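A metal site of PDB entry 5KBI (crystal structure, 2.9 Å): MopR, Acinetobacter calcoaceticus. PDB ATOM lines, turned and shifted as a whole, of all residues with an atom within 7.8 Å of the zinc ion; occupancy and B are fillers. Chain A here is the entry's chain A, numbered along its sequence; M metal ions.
The side-chain sulfur (SG) of Cys 189 sits close to the backbone NH (N) of Val 182.
The backbone NH of Cys 189 lies within hydrogen-bond range of the backbone carbonyl oxygen of Trp 134, 3.1 Å away.
The side-chain sulfur (SG) of Cys 155 sits close to the side-chain hydroxyl (OG) of Ser 137, 3.3 Å away.
The backbone NH (N) of Ala 154 lies close to the side-chain sulfur (SG) of Cys 181, 3.5 Å away.
The backbone NH of Ala 183 sits close to the side-chain sulfur of Cys 181 (3.2 Å).
The side-chain carboxylate (OD2) of Asp 186 lies within hydrogen-bond range of the backbone NH (N) of Cys 181 (2.7 Å).
The backbone NH (N) of Ala 140 sits at hydrogen-bond distance from the side-chain hydroxyl (OG) of Ser 137, 3.1 Å away.
Merely in contact with the zinc ion: Ala 140 and Val 182.
Six residues have an atom within 4 Å of the zinc ion: Ala 140, Cys 155, Glu 178, Cys 181, Val 182 and Cys 189.
Along chain A the residues within 4 Å of the zinc ion span positions 140 to 189.
The nearest printed residue that does not touch the zinc ion is Ser 137 (4.5 Å).
The zinc ion is bound by SG of Cys 189, OE2 of Glu 178, SG of Cys 155 and SG of Cys 181.
The zinc ion has four donor atoms within binding distance.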
ATOM      1  N   VAL A 112      -0.199 -27.633  -9.404  1.00  0.00           N
ATOM      2  CA  VAL A 112       1.237 -27.761  -9.272  1.00  0.00           C
ATOM      3  C   VAL A 112       1.933 -28.034 -10.610  1.00  0.00           C
ATOM      4  O   VAL A 112       1.352 -28.653 -11.520  1.00  0.00           O
ATOM      5  CB  VAL A 112       1.594 -28.851  -8.255  1.00  0.00           C
ATOM      6  CG1 VAL A 112       1.568 -30.225  -8.906  1.00  0.00           C
ATOM      7  CG2 VAL A 112       2.940 -28.520  -7.637  1.00  0.00           C
ATOM      8  N   TRP A 134       7.960 -30.725  -7.396  1.00  0.00           N
ATOM      9  CA  TRP A 134       6.753 -29.922  -7.464  1.00  0.00           C
ATOM     10  C   TRP A 134       7.147 -28.492  -7.357  1.00  0.00           C
ATOM     11  O   TRP A 134       7.798 -28.133  -6.387  1.00  0.00           O
ATOM     12  CB  TRP A 134       5.897 -30.258  -6.285  1.00  0.00           C
ATOM     13  CG  TRP A 134       5.018 -31.455  -6.508  1.00  0.00           C
ATOM     14  CD1 TRP A 134       4.646 -32.048  -7.728  1.00  0.00           C
ATOM     15  CD2 TRP A 134       4.303 -32.219  -5.477  1.00  0.00           C
ATOM     16  NE1 TRP A 134       3.799 -33.101  -7.506  1.00  0.00           N
ATOM     17  CE2 TRP A 134       3.550 -33.268  -6.191  1.00  0.00           C
ATOM     18  CE3 TRP A 134       4.222 -32.148  -4.079  1.00  0.00           C
ATOM     19  CZ2 TRP A 134       2.775 -34.192  -5.518  1.00  0.00           C
ATOM     20  CZ3 TRP A 134       3.437 -33.071  -3.420  1.00  0.00           C
ATOM     21  CH2 TRP A 134       2.721 -34.080  -4.125  1.00  0.00           C
ATOM     22  N   SER A 137       3.519 -25.061  -5.820  1.00  0.00           N
ATOM     23  CA  SER A 137       2.382 -25.758  -5.223  1.00  0.00           C
ATOM     24  C   SER A 137       1.498 -24.744  -4.569  1.00  0.00           C
ATOM     25  O   SER A 137       1.977 -23.868  -3.861  1.00  0.00           O
ATOM     26  CB  SER A 137       2.834 -26.728  -4.147  1.00  0.00           C
ATOM     27  OG  SER A 137       1.765 -26.954  -3.234  1.00  0.00           O
ATOM     28  N   PHE A 138       0.200 -24.855  -4.804  1.00  0.00           N
ATOM     29  CA  PHE A 138      -0.734 -23.906  -4.189  1.00  0.00           C
ATOM     30  C   PHE A 138      -0.833 -24.255  -2.722  1.00  0.00           C
ATOM     31  O   PHE A 138      -0.991 -23.387  -1.871  1.00  0.00           O
ATOM     32  CB  PHE A 138      -2.121 -23.965  -4.850  1.00  0.00           C
ATOM     33  CG  PHE A 138      -2.951 -25.125  -4.395  1.00  0.00           C
ATOM     34  CD1 PHE A 138      -2.850 -26.352  -5.034  1.00  0.00           C
ATOM     35  CD2 PHE A 138      -3.807 -24.997  -3.314  1.00  0.00           C
ATOM     36  CE1 PHE A 138      -3.616 -27.452  -4.620  1.00  0.00           C
ATOM     37  CE2 PHE A 138      -4.572 -26.074  -2.876  1.00  0.00           C
ATOM     38  CZ  PHE A 138      -4.474 -27.308  -3.543  1.00  0.00           C
ATOM     39  N   GLU A 139      -0.724 -25.552  -2.457  1.00  0.00           N
ATOM     40  CA  GLU A 139      -1.049 -26.144  -1.167  1.00  0.00           C
ATOM     41  C   GLU A 139      -0.078 -25.609  -0.137  1.00  0.00           C
ATOM     42  O   GLU A 139      -0.465 -25.093   0.904  1.00  0.00           O
ATOM     43  CB  GLU A 139      -1.031 -27.671  -1.270  1.00  0.00           C
ATOM     44  CG  GLU A 139      -1.954 -28.355  -0.273  1.00  0.00           C
ATOM     45  CD  GLU A 139      -2.385 -29.787  -0.617  1.00  0.00           C
ATOM     46  OE1 GLU A 139      -1.793 -30.452  -1.484  1.00  0.00           O
ATOM     47  OE2 GLU A 139      -3.314 -30.298   0.041  1.00  0.00           O
ATOM     48  N   ALA A 140       1.191 -25.662  -0.473  1.00  0.00           N
ATOM     49  CA  ALA A 140       2.217 -25.056   0.330  1.00  0.00           C
ATOM     50  C   ALA A 140       1.947 -23.563   0.560  1.00  0.00           C
ATOM     51  O   ALA A 140       2.131 -23.054   1.672  1.00  0.00           O
ATOM     52  CB  ALA A 140       3.569 -25.266  -0.334  1.00  0.00           C
ATOM     53  N   GLU A 141       1.482 -22.875  -0.471  1.00  0.00           N
ATOM     54  CA  GLU A 141       1.272 -21.431  -0.396  1.00  0.00           C
ATOM     55  C   GLU A 141       0.135 -21.121   0.546  1.00  0.00           C
ATOM     56  O   GLU A 141       0.260 -20.270   1.432  1.00  0.00           O
ATOM     57  CB  GLU A 141       0.984 -20.883  -1.784  1.00  0.00           C
ATOM     58  CG  GLU A 141       0.933 -19.370  -1.922  1.00  0.00           C
ATOM     59  CD  GLU A 141       0.353 -18.947  -3.289  1.00  0.00           C
ATOM     60  OE1 GLU A 141       0.689 -19.602  -4.323  1.00  0.00           O
ATOM     61  OE2 GLU A 141      -0.440 -17.954  -3.339  1.00  0.00           O
ATOM     62  N   GLN A 152       6.227 -30.242   9.216  1.00  0.00           N
ATOM     63  CA  GLN A 152       6.096 -31.389   8.311  1.00  0.00           C
ATOM     64  C   GLN A 152       5.739 -30.858   6.890  1.00  0.00           C
ATOM     65  O   GLN A 152       5.462 -29.652   6.742  1.00  0.00           O
ATOM     66  CB  GLN A 152       5.045 -32.367   8.848  1.00  0.00           C
ATOM     67  CG  GLN A 152       3.746 -31.691   9.328  1.00  0.00           C
ATOM     68  CD  GLN A 152       2.743 -32.639  10.014  1.00  0.00           C
ATOM     69  OE1 GLN A 152       1.914 -33.296   9.349  1.00  0.00           O
ATOM     70  NE2 GLN A 152       2.792 -32.686  11.354  1.00  0.00           N
ATOM     71  N   PRO A 153       5.770 -31.717   5.846  1.00  0.00           N
ATOM     72  CA  PRO A 153       5.365 -31.199   4.541  1.00  0.00           C
ATOM     73  C   PRO A 153       3.869 -30.913   4.525  1.00  0.00           C
ATOM     74  O   PRO A 153       3.158 -31.540   5.262  1.00  0.00           O
ATOM     75  CB  PRO A 153       5.668 -32.352   3.589  1.00  0.00           C
ATOM     76  CG  PRO A 153       5.690 -33.576   4.422  1.00  0.00           C
ATOM     77  CD  PRO A 153       6.246 -33.117   5.735  1.00  0.00           C
ATOM     78  N   ALA A 154       3.400 -29.968   3.712  1.00  0.00           N
ATOM     79  CA  ALA A 154       1.978 -29.623   3.646  1.00  0.00           C
ATOM     80  C   ALA A 154       1.137 -30.208   2.463  1.00  0.00           C
ATOM     81  O   ALA A 154      -0.100 -30.165   2.477  1.00  0.00           O
ATOM     82  CB  ALA A 154       1.824 -28.133   3.647  1.00  0.00           C
ATOM     83  N   CYS A 155       1.796 -30.759   1.454  1.00  0.00           N
ATOM     84  CA  CYS A 155       1.122 -31.007   0.192  1.00  0.00           C
ATOM     85  C   CYS A 155       0.346 -32.331   0.082  1.00  0.00           C
ATOM     86  O   CYS A 155       0.483 -33.073  -0.890  1.00  0.00           O
ATOM     87  CB  CYS A 155       2.090 -30.811  -0.959  1.00  0.00           C
ATOM     88  SG  CYS A 155       2.757 -29.142  -0.977  1.00  0.00           S
ATOM     89  N   TRP A 156      -0.506 -32.525   1.076  1.00  0.00           N
ATOM     90  CA  TRP A 156      -1.334 -33.685   1.240  1.00  0.00           C
ATOM     91  C   TRP A 156      -2.197 -34.040   0.057  1.00  0.00           C
ATOM     92  O   TRP A 156      -2.300 -35.234  -0.322  1.00  0.00           O
ATOM     93  CB  TRP A 156      -2.229 -33.477   2.452  1.00  0.00           C
ATOM     94  CG  TRP A 156      -1.536 -32.867   3.608  1.00  0.00           C
ATOM     95  CD1 TRP A 156      -0.186 -32.986   3.935  1.00  0.00           C
ATOM     96  CD2 TRP A 156      -2.102 -32.031   4.673  1.00  0.00           C
ATOM     97  NE1 TRP A 156       0.100 -32.291   5.081  1.00  0.00           N
ATOM     98  CE2 TRP A 156      -0.998 -31.688   5.573  1.00  0.00           C
ATOM     99  CE3 TRP A 156      -3.361 -31.550   4.953  1.00  0.00           C
ATOM    100  CZ2 TRP A 156      -1.168 -30.893   6.712  1.00  0.00           C
ATOM    101  CZ3 TRP A 156      -3.532 -30.756   6.092  1.00  0.00           C
ATOM    102  CH2 TRP A 156      -2.454 -30.440   6.957  1.00  0.00           C
ATOM    103  N   LEU A 158      -2.256 -32.854  -3.241  1.00  0.00           N
ATOM    104  CA  LEU A 158      -1.319 -33.117  -4.313  1.00  0.00           C
ATOM    105  C   LEU A 158      -0.680 -34.480  -4.149  1.00  0.00           C
ATOM    106  O   LEU A 158      -0.448 -35.184  -5.140  1.00  0.00           O
ATOM    107  CB  LEU A 158      -0.228 -32.072  -4.323  1.00  0.00           C
ATOM    108  CG  LEU A 158      -0.675 -30.630  -4.509  1.00  0.00           C
ATOM    109  CD1 LEU A 158       0.522 -29.687  -4.637  1.00  0.00           C
ATOM    110  CD2 LEU A 158      -1.620 -30.495  -5.702  1.00  0.00           C
ATOM    111  N   GLU A 178       6.747 -36.795   0.403  1.00  0.00           N
ATOM    112  CA  GLU A 178       7.193 -35.406   0.099  1.00  0.00           C
ATOM    113  C   GLU A 178       8.529 -35.157   0.860  1.00  0.00           C
ATOM    114  O   GLU A 178       8.532 -34.967   2.055  1.00  0.00           O
ATOM    115  CB  GLU A 178       6.091 -34.338   0.339  1.00  0.00           C
ATOM    116  CG  GLU A 178       6.419 -32.953  -0.266  1.00  0.00           C
ATOM    117  CD  GLU A 178       5.332 -31.851  -0.144  1.00  0.00           C
ATOM    118  OE1 GLU A 178       4.514 -31.823   0.795  1.00  0.00           O
ATOM    119  OE2 GLU A 178       5.309 -30.952  -0.997  1.00  0.00           O
ATOM    120  N   HIS A 180      10.909 -32.637   0.315  1.00  0.00           N
ATOM    121  CA  HIS A 180      11.132 -31.235   0.664  1.00  0.00           C
ATOM    122  C   HIS A 180       9.908 -30.501   0.322  1.00  0.00           C
ATOM    123  O   HIS A 180       9.280 -30.807  -0.684  1.00  0.00           O
ATOM    124  CB  HIS A 180      12.262 -30.603  -0.144  1.00  0.00           C
ATOM    125  CG  HIS A 180      13.605 -31.231   0.082  1.00  0.00           C
ATOM    126  ND1 HIS A 180      13.952 -31.836   1.229  1.00  0.00           N
ATOM    127  CD2 HIS A 180      14.725 -31.315  -0.743  1.00  0.00           C
ATOM    128  CE1 HIS A 180      15.195 -32.309   1.145  1.00  0.00           C
ATOM    129  NE2 HIS A 180      15.683 -31.979  -0.063  1.00  0.00           N
ATOM    130  N   CYS A 181       9.559 -29.506   1.132  1.00  0.00           N
ATOM    131  CA  CYS A 181       8.319 -28.768   0.915  1.00  0.00           C
ATOM    132  C   CYS A 181       8.470 -27.246   1.134  1.00  0.00           C
ATOM    133  O   CYS A 181       9.081 -26.799   2.109  1.00  0.00           O
ATOM    134  CB  CYS A 181       7.180 -29.336   1.775  1.00  0.00           C
ATOM    135  SG  CYS A 181       5.623 -28.447   1.531  1.00  0.00           S
ATOM    136  N   VAL A 182       7.923 -26.454   0.218  1.00  0.00           N
ATOM    137  CA  VAL A 182       7.968 -25.029   0.375  1.00  0.00           C
ATOM    138  C   VAL A 182       7.439 -24.658   1.762  1.00  0.00           C
ATOM    139  O   VAL A 182       7.860 -23.656   2.358  1.00  0.00           O
ATOM    140  CB  VAL A 182       7.182 -24.350  -0.740  1.00  0.00           C
ATOM    141  CG1 VAL A 182       6.555 -23.074  -0.288  1.00  0.00           C
ATOM    142  CG2 VAL A 182       8.097 -24.069  -1.891  1.00  0.00           C
ATOM    143  N   ALA A 183       6.551 -25.509   2.290  1.00  0.00           N
ATOM    144  CA  ALA A 183       5.939 -25.220   3.573  1.00  0.00           C
ATOM    145  C   ALA A 183       7.001 -25.181   4.613  1.00  0.00           C
ATOM    146  O   ALA A 183       6.982 -24.369   5.521  1.00  0.00           O
ATOM    147  CB  ALA A 183       4.937 -26.288   3.907  1.00  0.00           C
ATOM    148  N   GLN A 184       7.944 -26.098   4.485  1.00  0.00           N
ATOM    149  CA  GLN A 184       9.044 -26.232   5.429  1.00  0.00           C
ATOM    150  C   GLN A 184      10.212 -25.272   5.147  1.00  0.00           C
ATOM    151  O   GLN A 184      11.183 -25.306   5.885  1.00  0.00           O
ATOM    152  CB  GLN A 184       9.553 -27.663   5.432  1.00  0.00           C
ATOM    153  CG  GLN A 184       8.524 -28.688   5.883  1.00  0.00           C
ATOM    154  CD  GLN A 184       9.102 -30.100   5.955  1.00  0.00           C
ATOM    155  OE1 GLN A 184       8.565 -31.041   5.370  1.00  0.00           O
ATOM    156  NE2 GLN A 184      10.215 -30.247   6.675  1.00  0.00           N
ATOM    157  N   ASP A 186      12.016 -25.077   2.269  1.00  0.00           N
ATOM    158  CA  ASP A 186      12.715 -25.577   1.078  1.00  0.00           C
ATOM    159  C   ASP A 186      12.415 -24.774  -0.178  1.00  0.00           C
ATOM    160  O   ASP A 186      11.314 -24.302  -0.348  1.00  0.00           O
ATOM    161  CB  ASP A 186      12.263 -26.996   0.849  1.00  0.00           C
ATOM    162  CG  ASP A 186      12.631 -27.926   1.997  1.00  0.00           C
ATOM    163  OD1 ASP A 186      13.800 -27.874   2.426  1.00  0.00           O
ATOM    164  OD2 ASP A 186      11.766 -28.710   2.449  1.00  0.00           O
ATOM    165  N   HIS A 188      11.937 -25.539  -3.439  1.00  0.00           N
ATOM    166  CA  HIS A 188      10.841 -26.082  -4.178  1.00  0.00           C
ATOM    167  C   HIS A 188      10.403 -27.210  -3.345  1.00  0.00           C
ATOM    168  O   HIS A 188      10.973 -27.428  -2.279  1.00  0.00           O
ATOM    169  CB  HIS A 188      11.232 -26.490  -5.609  1.00  0.00           C
ATOM    170  CG  HIS A 188      12.594 -27.209  -5.714  1.00  0.00           C
ATOM    171  ND1 HIS A 188      12.773 -28.522  -5.408  1.00  0.00           N
ATOM    172  CD2 HIS A 188      13.845 -26.731  -6.134  1.00  0.00           C
ATOM    173  CE1 HIS A 188      14.062 -28.872  -5.590  1.00  0.00           C
ATOM    174  NE2 HIS A 188      14.719 -27.779  -6.035  1.00  0.00           N
ATOM    175  N   CYS A 189       9.364 -27.924  -3.774  1.00  0.00           N
ATOM    176  CA  CYS A 189       8.835 -29.091  -3.039  1.00  0.00           C
ATOM    177  C   CYS A 189       9.443 -30.287  -3.763  1.00  0.00           C
ATOM    178  O   CYS A 189       9.787 -30.146  -4.929  1.00  0.00           O
ATOM    179  CB  CYS A 189       7.284 -29.139  -3.075  1.00  0.00           C
ATOM    180  SG  CYS A 189       6.377 -27.995  -1.968  1.00  0.00           S
ATOM    181  N   ARG A 190       9.587 -31.442  -3.111  1.00  0.00           N
ATOM    182  CA  ARG A 190       9.955 -32.611  -3.884  1.00  0.00           C
ATOM    183  C   ARG A 190       9.416 -33.943  -3.351  1.00  0.00           C
ATOM    184  O   ARG A 190       9.445 -34.202  -2.158  1.00  0.00           O
ATOM    185  CB  ARG A 190      11.468 -32.680  -4.094  1.00  0.00           C
ATOM    186  CG  ARG A 190      11.997 -34.025  -4.616  1.00  0.00           C
ATOM    187  CD  ARG A 190      13.383 -33.894  -5.217  1.00  0.00           C
ATOM    188  NE  ARG A 190      14.233 -34.970  -4.731  1.00  0.00           N
ATOM    189  CZ  ARG A 190      15.417 -35.268  -5.265  1.00  0.00           C
ATOM    190  NH1 ARG A 190      15.872 -34.561  -6.288  1.00  0.00           N
ATOM    191  NH2 ARG A 190      16.126 -36.288  -4.779  1.00  0.00           N
ATOM    192  N   ILE A 191       8.965 -34.789  -4.280  1.00  0.00           N
ATOM    193  CA  ILE A 191       8.434 -36.103  -3.934  1.00  0.00           C
ATOM    194  C   ILE A 191       9.184 -37.255  -4.551  1.00  0.00           C
ATOM    195  O   ILE A 191       9.899 -37.094  -5.575  1.00  0.00           O
ATOM    196  CB  ILE A 191       6.976 -36.258  -4.341  1.00  0.00           C
ATOM    197  CG1 ILE A 191       6.762 -35.763  -5.753  1.00  0.00           C
ATOM    198  CG2 ILE A 191       6.088 -35.491  -3.389  1.00  0.00           C
ATOM    199  CD1 ILE A 191       5.825 -36.642  -6.554  1.00  0.00           C
HETATM  200 ZN    ZN M   1       4.906 -28.824  -0.536  1.00  0.00          ZN
